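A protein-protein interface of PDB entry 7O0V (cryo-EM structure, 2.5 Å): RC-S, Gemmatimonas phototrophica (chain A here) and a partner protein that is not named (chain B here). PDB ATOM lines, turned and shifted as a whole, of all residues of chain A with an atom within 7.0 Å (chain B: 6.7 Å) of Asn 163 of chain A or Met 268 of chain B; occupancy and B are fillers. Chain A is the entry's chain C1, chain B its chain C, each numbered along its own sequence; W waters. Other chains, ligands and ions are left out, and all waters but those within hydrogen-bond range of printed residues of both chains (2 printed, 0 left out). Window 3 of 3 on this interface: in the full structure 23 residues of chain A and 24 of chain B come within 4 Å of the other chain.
Of the 9 printed residues of chain A, 4 touch a printed residue of chain B. Hydrophobic or aromatic side chains of chain A that line the printed part of chain B: Ala 159 and Tyr 190. Along chain A the printed residues that touch a printed residue of chain B span positions 159 to 190. Printed residues of chain B that touch a printed residue of chain A: Ser 163, Ser 164, Gln 165 and Met 268. Hydrophobic or aromatic side chains of chain B within 4 Å of the printed part of chain A: Met 268. Among the printed residues, 6 pairs touch across the chains. Among the printed residues, no Asp or Glu carboxylate lies within 4 Å of a Lys or Arg side-chain nitrogen of the other chain.
Water W1 lies within hydrogen-bond range of OG of Ser 163 of chain B, NH2 of Arg 165 of chain A, OH of Tyr 190 of chain A and OG of Ser 164 of chain B. Water W2 lies within hydrogen-bond range of O of Asn 163 of chain A (2.8 Å) and N of Gln 165 of chain B (2.9 Å).
The backbone carbonyl oxygen (O) of Ala 159 of chain A lies within hydrogen-bond range of the side-chain amide nitrogen (NE2) of Gln 164 of chain A (3.0 Å).
NE of Arg 165 of chain A sits at hydrogen-bond distance from OG of Ser 164 of chain B (2.9 Å). The side-chain amide nitrogen (ND2) of Asn 163 of chain A lies within hydrogen-bond range of the backbone carbonyl oxygen (O) of Ser 163 of chain B. ND2 of Asn 163 of chain A is in hydrogen-bond range of SD of Met 268 of chain B.
Asn 163 of chain A touches just these residues of chain B: Ser 163, Ser 164 and Met 268. Of chain A, only Asn 163 (3.5 Å) comes within 4 Å of Met 268 of chain B. Of the printed residues of chain A, Ser 163 of chain B touches Asn 163 and Tyr 190. Of the printed residues of chain A, Ser 164 of chain B touches Asn 163 (3.3 Å) and Arg 165 (2.9 Å). Printed residues of chain A within 4 Å of Gln 165 of chain B: Ala 159. Of the printed residues of chain B, Tyr 190 of chain A touches Ser 163 (3.6 Å). Printed residues of chain B within 4 Å of Ala 159 of chain A: Gln 165.
Ala 159 of chain A touches Gln 165 of chain B. Asn 163 of chain A touches Ser 164 of chain B. OH of Tyr 190 of chain A touches CB of Ser 163 of chain B, at 3.6 Å.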
ATOM      1  N   ALA A 159     -24.947  25.214 -14.901  1.00  0.00           N
ATOM      2  CA  ALA A 159     -23.587  25.169 -14.392  1.00  0.00           C
ATOM      3  C   ALA A 159     -22.627  24.702 -15.487  1.00  0.00           C
ATOM      4  O   ALA A 159     -23.047  24.075 -16.463  1.00  0.00           O
ATOM      5  CB  ALA A 159     -23.510  24.235 -13.186  1.00  0.00           C
ATOM      6  N   PRO A 160     -21.333  25.008 -15.359  1.00  0.00           N
ATOM      7  CA  PRO A 160     -20.333  24.312 -16.180  1.00  0.00           C
ATOM      8  C   PRO A 160     -20.517  22.803 -16.086  1.00  0.00           C
ATOM      9  O   PRO A 160     -20.924  22.275 -15.049  1.00  0.00           O
ATOM     10  CB  PRO A 160     -18.996  24.764 -15.577  1.00  0.00           C
ATOM     11  CG  PRO A 160     -19.306  26.058 -14.910  1.00  0.00           C
ATOM     12  CD  PRO A 160     -20.701  25.910 -14.383  1.00  0.00           C
ATOM     13  N   ILE A 161     -20.218  22.105 -17.184  1.00  0.00           N
ATOM     14  CA  ILE A 161     -20.491  20.670 -17.234  1.00  0.00           C
ATOM     15  C   ILE A 161     -19.714  19.914 -16.161  1.00  0.00           C
ATOM     16  O   ILE A 161     -20.180  18.885 -15.657  1.00  0.00           O
ATOM     17  CB  ILE A 161     -20.214  20.116 -18.648  1.00  0.00           C
ATOM     18  CG1 ILE A 161     -20.917  18.769 -18.834  1.00  0.00           C
ATOM     19  CG2 ILE A 161     -18.723  20.002 -18.923  1.00  0.00           C
ATOM     20  CD1 ILE A 161     -20.822  18.215 -20.234  1.00  0.00           C
ATOM     21  N   THR A 162     -18.534  20.411 -15.781  1.00  0.00           N
ATOM     22  CA  THR A 162     -17.752  19.830 -14.694  1.00  0.00           C
ATOM     23  C   THR A 162     -18.384  19.996 -13.316  1.00  0.00           C
ATOM     24  O   THR A 162     -17.883  19.404 -12.355  1.00  0.00           O
ATOM     25  CB  THR A 162     -16.348  20.435 -14.683  1.00  0.00           C
ATOM     26  OG1 THR A 162     -16.441  21.862 -14.759  1.00  0.00           O
ATOM     27  CG2 THR A 162     -15.540  19.919 -15.861  1.00  0.00           C
ATOM     28  N   ASN A 163     -19.456  20.776 -13.188  1.00  0.00           N
ATOM     29  CA  ASN A 163     -20.195  20.878 -11.935  1.00  0.00           C
ATOM     30  C   ASN A 163     -21.527  20.140 -11.964  1.00  0.00           C
ATOM     31  O   ASN A 163     -22.320  20.276 -11.027  1.00  0.00           O
ATOM     32  CB  ASN A 163     -20.414  22.350 -11.580  1.00  0.00           C
ATOM     33  CG  ASN A 163     -19.115  23.082 -11.319  1.00  0.00           C
ATOM     34  OD1 ASN A 163     -18.487  23.601 -12.239  1.00  0.00           O
ATOM     35  ND2 ASN A 163     -18.704  23.123 -10.059  1.00  0.00           N
ATOM     36  N   GLN A 164     -21.796  19.375 -13.013  1.00  0.00           N
ATOM     37  CA  GLN A 164     -23.045  18.642 -13.161  1.00  0.00           C
ATOM     38  C   GLN A 164     -22.840  17.201 -12.702  1.00  0.00           C
ATOM     39  O   GLN A 164     -21.910  16.529 -13.159  1.00  0.00           O
ATOM     40  CB  GLN A 164     -23.520  18.708 -14.614  1.00  0.00           C
ATOM     41  CG  GLN A 164     -23.829  20.139 -15.058  1.00  0.00           C
ATOM     42  CD  GLN A 164     -24.324  20.238 -16.487  1.00  0.00           C
ATOM     43  OE1 GLN A 164     -24.895  19.295 -17.025  1.00  0.00           O
ATOM     44  NE2 GLN A 164     -24.101  21.389 -17.111  1.00  0.00           N
ATOM     45  N   ARG A 165     -23.696  16.736 -11.793  1.00  0.00           N
ATOM     46  CA  ARG A 165     -23.588  15.369 -11.294  1.00  0.00           C
ATOM     47  C   ARG A 165     -24.025  14.362 -12.351  1.00  0.00           C
ATOM     48  O   ARG A 165     -25.042  14.544 -13.023  1.00  0.00           O
ATOM     49  CB  ARG A 165     -24.451  15.186 -10.047  1.00  0.00           C
ATOM     50  CG  ARG A 165     -23.985  15.914  -8.808  1.00  0.00           C
ATOM     51  CD  ARG A 165     -24.948  15.636  -7.666  1.00  0.00           C
ATOM     52  NE  ARG A 165     -24.584  16.334  -6.440  1.00  0.00           N
ATOM     53  CZ  ARG A 165     -25.195  16.166  -5.277  1.00  0.00           C
ATOM     54  NH1 ARG A 165     -26.235  15.358  -5.152  1.00  0.00           N
ATOM     55  NH2 ARG A 165     -24.763  16.838  -4.214  1.00  0.00           N
ATOM     56  N   TYR A 190     -18.741  13.552 -11.316  1.00  0.00           N
ATOM     57  CA  TYR A 190     -19.083  14.673 -12.178  1.00  0.00           C
ATOM     58  C   TYR A 190     -18.678  14.375 -13.615  1.00  0.00           C
ATOM     59  O   TYR A 190     -17.787  13.563 -13.875  1.00  0.00           O
ATOM     60  CB  TYR A 190     -18.438  15.968 -11.670  1.00  0.00           C
ATOM     61  CG  TYR A 190     -18.841  16.262 -10.246  1.00  0.00           C
ATOM     62  CD1 TYR A 190     -20.050  16.881  -9.960  1.00  0.00           C
ATOM     63  CD2 TYR A 190     -18.043  15.867  -9.183  1.00  0.00           C
ATOM     64  CE1 TYR A 190     -20.432  17.137  -8.659  1.00  0.00           C
ATOM     65  CE2 TYR A 190     -18.420  16.108  -7.879  1.00  0.00           C
ATOM     66  CZ  TYR A 190     -19.614  16.744  -7.622  1.00  0.00           C
ATOM     67  OH  TYR A 190     -19.994  16.980  -6.322  1.00  0.00           O
ATOM     68  N   TYR A 191     -19.352  15.039 -14.546  1.00  0.00           N
ATOM     69  CA  TYR A 191     -18.972  14.936 -15.946  1.00  0.00           C
ATOM     70  C   TYR A 191     -17.593  15.549 -16.176  1.00  0.00           C
ATOM     71  O   TYR A 191     -17.252  16.567 -15.567  1.00  0.00           O
ATOM     72  CB  TYR A 191     -20.013  15.630 -16.823  1.00  0.00           C
ATOM     73  CG  TYR A 191     -21.295  14.845 -16.937  1.00  0.00           C
ATOM     74  CD1 TYR A 191     -21.417  13.806 -17.850  1.00  0.00           C
ATOM     75  CD2 TYR A 191     -22.372  15.116 -16.107  1.00  0.00           C
ATOM     76  CE1 TYR A 191     -22.585  13.082 -17.953  1.00  0.00           C
ATOM     77  CE2 TYR A 191     -23.542  14.390 -16.196  1.00  0.00           C
ATOM     78  CZ  TYR A 191     -23.644  13.377 -17.122  1.00  0.00           C
ATOM     79  OH  TYR A 191     -24.806  12.646 -17.212  1.00  0.00           O
ATOM     80  N   PHE B 161     -16.524  23.356  -0.151  1.00  0.00           N
ATOM     81  CA  PHE B 161     -16.374  24.247  -1.290  1.00  0.00           C
ATOM     82  C   PHE B 161     -17.542  24.042  -2.245  1.00  0.00           C
ATOM     83  O   PHE B 161     -18.268  23.049  -2.160  1.00  0.00           O
ATOM     84  CB  PHE B 161     -15.053  23.990  -2.026  1.00  0.00           C
ATOM     85  CG  PHE B 161     -13.844  24.055  -1.141  1.00  0.00           C
ATOM     86  CD1 PHE B 161     -13.234  25.264  -0.861  1.00  0.00           C
ATOM     87  CD2 PHE B 161     -13.328  22.903  -0.571  1.00  0.00           C
ATOM     88  CE1 PHE B 161     -12.124  25.320  -0.046  1.00  0.00           C
ATOM     89  CE2 PHE B 161     -12.222  22.956   0.251  1.00  0.00           C
ATOM     90  CZ  PHE B 161     -11.621  24.166   0.514  1.00  0.00           C
ATOM     91  N   TYR B 162     -17.722  25.002  -3.151  1.00  0.00           N
ATOM     92  CA  TYR B 162     -18.674  24.828  -4.241  1.00  0.00           C
ATOM     93  C   TYR B 162     -18.406  23.542  -5.011  1.00  0.00           C
ATOM     94  O   TYR B 162     -17.260  23.180  -5.281  1.00  0.00           O
ATOM     95  CB  TYR B 162     -18.624  26.013  -5.205  1.00  0.00           C
ATOM     96  CG  TYR B 162     -18.999  27.340  -4.599  1.00  0.00           C
ATOM     97  CD1 TYR B 162     -20.030  27.439  -3.678  1.00  0.00           C
ATOM     98  CD2 TYR B 162     -18.340  28.501  -4.972  1.00  0.00           C
ATOM     99  CE1 TYR B 162     -20.389  28.658  -3.139  1.00  0.00           C
ATOM    100  CE2 TYR B 162     -18.684  29.720  -4.431  1.00  0.00           C
ATOM    101  CZ  TYR B 162     -19.710  29.794  -3.518  1.00  0.00           C
ATOM    102  OH  TYR B 162     -20.044  31.008  -2.970  1.00  0.00           O
ATOM    103  N   SER B 163     -19.492  22.860  -5.365  1.00  0.00           N
ATOM    104  CA  SER B 163     -19.459  21.606  -6.102  1.00  0.00           C
ATOM    105  C   SER B 163     -20.595  21.634  -7.115  1.00  0.00           C
ATOM    106  O   SER B 163     -20.472  22.285  -8.158  1.00  0.00           O
ATOM    107  CB  SER B 163     -19.554  20.402  -5.161  1.00  0.00           C
ATOM    108  OG  SER B 163     -20.782  20.380  -4.460  1.00  0.00           O
ATOM    109  N   SER B 164     -21.704  20.961  -6.833  1.00  0.00           N
ATOM    110  CA  SER B 164     -22.874  21.073  -7.691  1.00  0.00           C
ATOM    111  C   SER B 164     -23.925  21.991  -7.070  1.00  0.00           C
ATOM    112  O   SER B 164     -23.870  22.350  -5.893  1.00  0.00           O
ATOM    113  CB  SER B 164     -23.460  19.689  -7.977  1.00  0.00           C
ATOM    114  OG  SER B 164     -24.038  19.130  -6.814  1.00  0.00           O
ATOM    115  N   GLN B 165     -24.894  22.374  -7.905  1.00  0.00           N
ATOM    116  CA  GLN B 165     -25.987  23.247  -7.477  1.00  0.00           C
ATOM    117  C   GLN B 165     -26.829  22.655  -6.347  1.00  0.00           C
ATOM    118  O   GLN B 165     -27.283  23.389  -5.463  1.00  0.00           O
ATOM    119  CB  GLN B 165     -26.874  23.575  -8.678  1.00  0.00           C
ATOM    120  CG  GLN B 165     -26.186  24.422  -9.735  1.00  0.00           C
ATOM    121  CD  GLN B 165     -27.063  24.674 -10.946  1.00  0.00           C
ATOM    122  OE1 GLN B 165     -28.099  24.033 -11.119  1.00  0.00           O
ATOM    123  NE2 GLN B 165     -26.647  25.604 -11.794  1.00  0.00           N
ATOM    124  N   GLN B 257     -11.748  35.030   0.324  1.00  0.00           N
ATOM    125  CA  GLN B 257     -11.260  34.512  -0.955  1.00  0.00           C
ATOM    126  C   GLN B 257      -9.999  35.188  -1.490  1.00  0.00           C
ATOM    127  O   GLN B 257      -9.078  34.469  -1.909  1.00  0.00           O
ATOM    128  CB  GLN B 257     -12.422  34.603  -1.952  1.00  0.00           C
ATOM    129  CG  GLN B 257     -12.149  34.080  -3.340  1.00  0.00           C
ATOM    130  CD  GLN B 257     -13.401  34.105  -4.193  1.00  0.00           C
ATOM    131  OE1 GLN B 257     -14.310  33.298  -4.002  1.00  0.00           O
ATOM    132  NE2 GLN B 257     -13.465  35.049  -5.122  1.00  0.00           N
ATOM    133  N   LEU B 265      -7.824  27.314  -1.604  1.00  0.00           N
ATOM    134  CA  LEU B 265      -9.082  27.556  -2.294  1.00  0.00           C
ATOM    135  C   LEU B 265      -9.613  26.298  -2.980  1.00  0.00           C
ATOM    136  O   LEU B 265      -8.873  25.359  -3.279  1.00  0.00           O
ATOM    137  CB  LEU B 265      -8.911  28.677  -3.317  1.00  0.00           C
ATOM    138  CG  LEU B 265      -8.395  29.994  -2.738  1.00  0.00           C
ATOM    139  CD1 LEU B 265      -8.269  31.046  -3.824  1.00  0.00           C
ATOM    140  CD2 LEU B 265      -9.302  30.483  -1.623  1.00  0.00           C
ATOM    141  N   GLY B 266     -10.922  26.294  -3.219  1.00  0.00           N
ATOM    142  CA  GLY B 266     -11.573  25.225  -3.949  1.00  0.00           C
ATOM    143  C   GLY B 266     -11.284  25.274  -5.440  1.00  0.00           C
ATOM    144  O   GLY B 266     -10.627  26.176  -5.960  1.00  0.00           O
ATOM    145  N   ALA B 267     -11.799  24.260  -6.143  1.00  0.00           N
ATOM    146  CA  ALA B 267     -11.633  24.204  -7.594  1.00  0.00           C
ATOM    147  C   ALA B 267     -12.308  25.374  -8.302  1.00  0.00           C
ATOM    148  O   ALA B 267     -11.799  25.852  -9.321  1.00  0.00           O
ATOM    149  CB  ALA B 267     -12.178  22.880  -8.129  1.00  0.00           C
ATOM    150  N   MET B 268     -13.443  25.848  -7.790  1.00  0.00           N
ATOM    151  CA  MET B 268     -14.052  27.073  -8.296  1.00  0.00           C
ATOM    152  C   MET B 268     -13.333  28.334  -7.834  1.00  0.00           C
ATOM    153  O   MET B 268     -13.747  29.435  -8.210  1.00  0.00           O
ATOM    154  CB  MET B 268     -15.526  27.142  -7.881  1.00  0.00           C
ATOM    155  CG  MET B 268     -16.370  25.964  -8.349  1.00  0.00           C
ATOM    156  SD  MET B 268     -16.396  25.762 -10.141  1.00  0.00           S
ATOM    157  CE  MET B 268     -17.431  27.141 -10.626  1.00  0.00           C
ATOM    158  N   GLY B 269     -12.277  28.205  -7.034  1.00  0.00           N
ATOM    159  CA  GLY B 269     -11.587  29.347  -6.471  1.00  0.00           C
ATOM    160  C   GLY B 269     -12.265  29.974  -5.275  1.00  0.00           C
ATOM    161  O   GLY B 269     -11.898  31.090  -4.888  1.00  0.00           O
ATOM    162  N   ASP B 270     -13.243  29.298  -4.682  1.00  0.00           N
ATOM    163  CA  ASP B 270     -13.957  29.811  -3.522  1.00  0.00           C
ATOM    164  C   ASP B 270     -13.208  29.524  -2.223  1.00  0.00           C
ATOM    165  O   ASP B 270     -12.416  28.584  -2.128  1.00  0.00           O
ATOM    166  CB  ASP B 270     -15.368  29.230  -3.471  1.00  0.00           C
ATOM    167  CG  ASP B 270     -15.379  27.720  -3.405  1.00  0.00           C
ATOM    168  OD1 ASP B 270     -14.779  27.077  -4.290  1.00  0.00           O
ATOM    169  OD2 ASP B 270     -16.007  27.176  -2.477  1.00  0.00           O
HETATM  170  O   HOH W   1     -22.165  18.091  -4.129  1.00  0.00           O
HETATM  171  O   HOH W   2     -24.769  21.564 -10.665  1.00  0.00           O
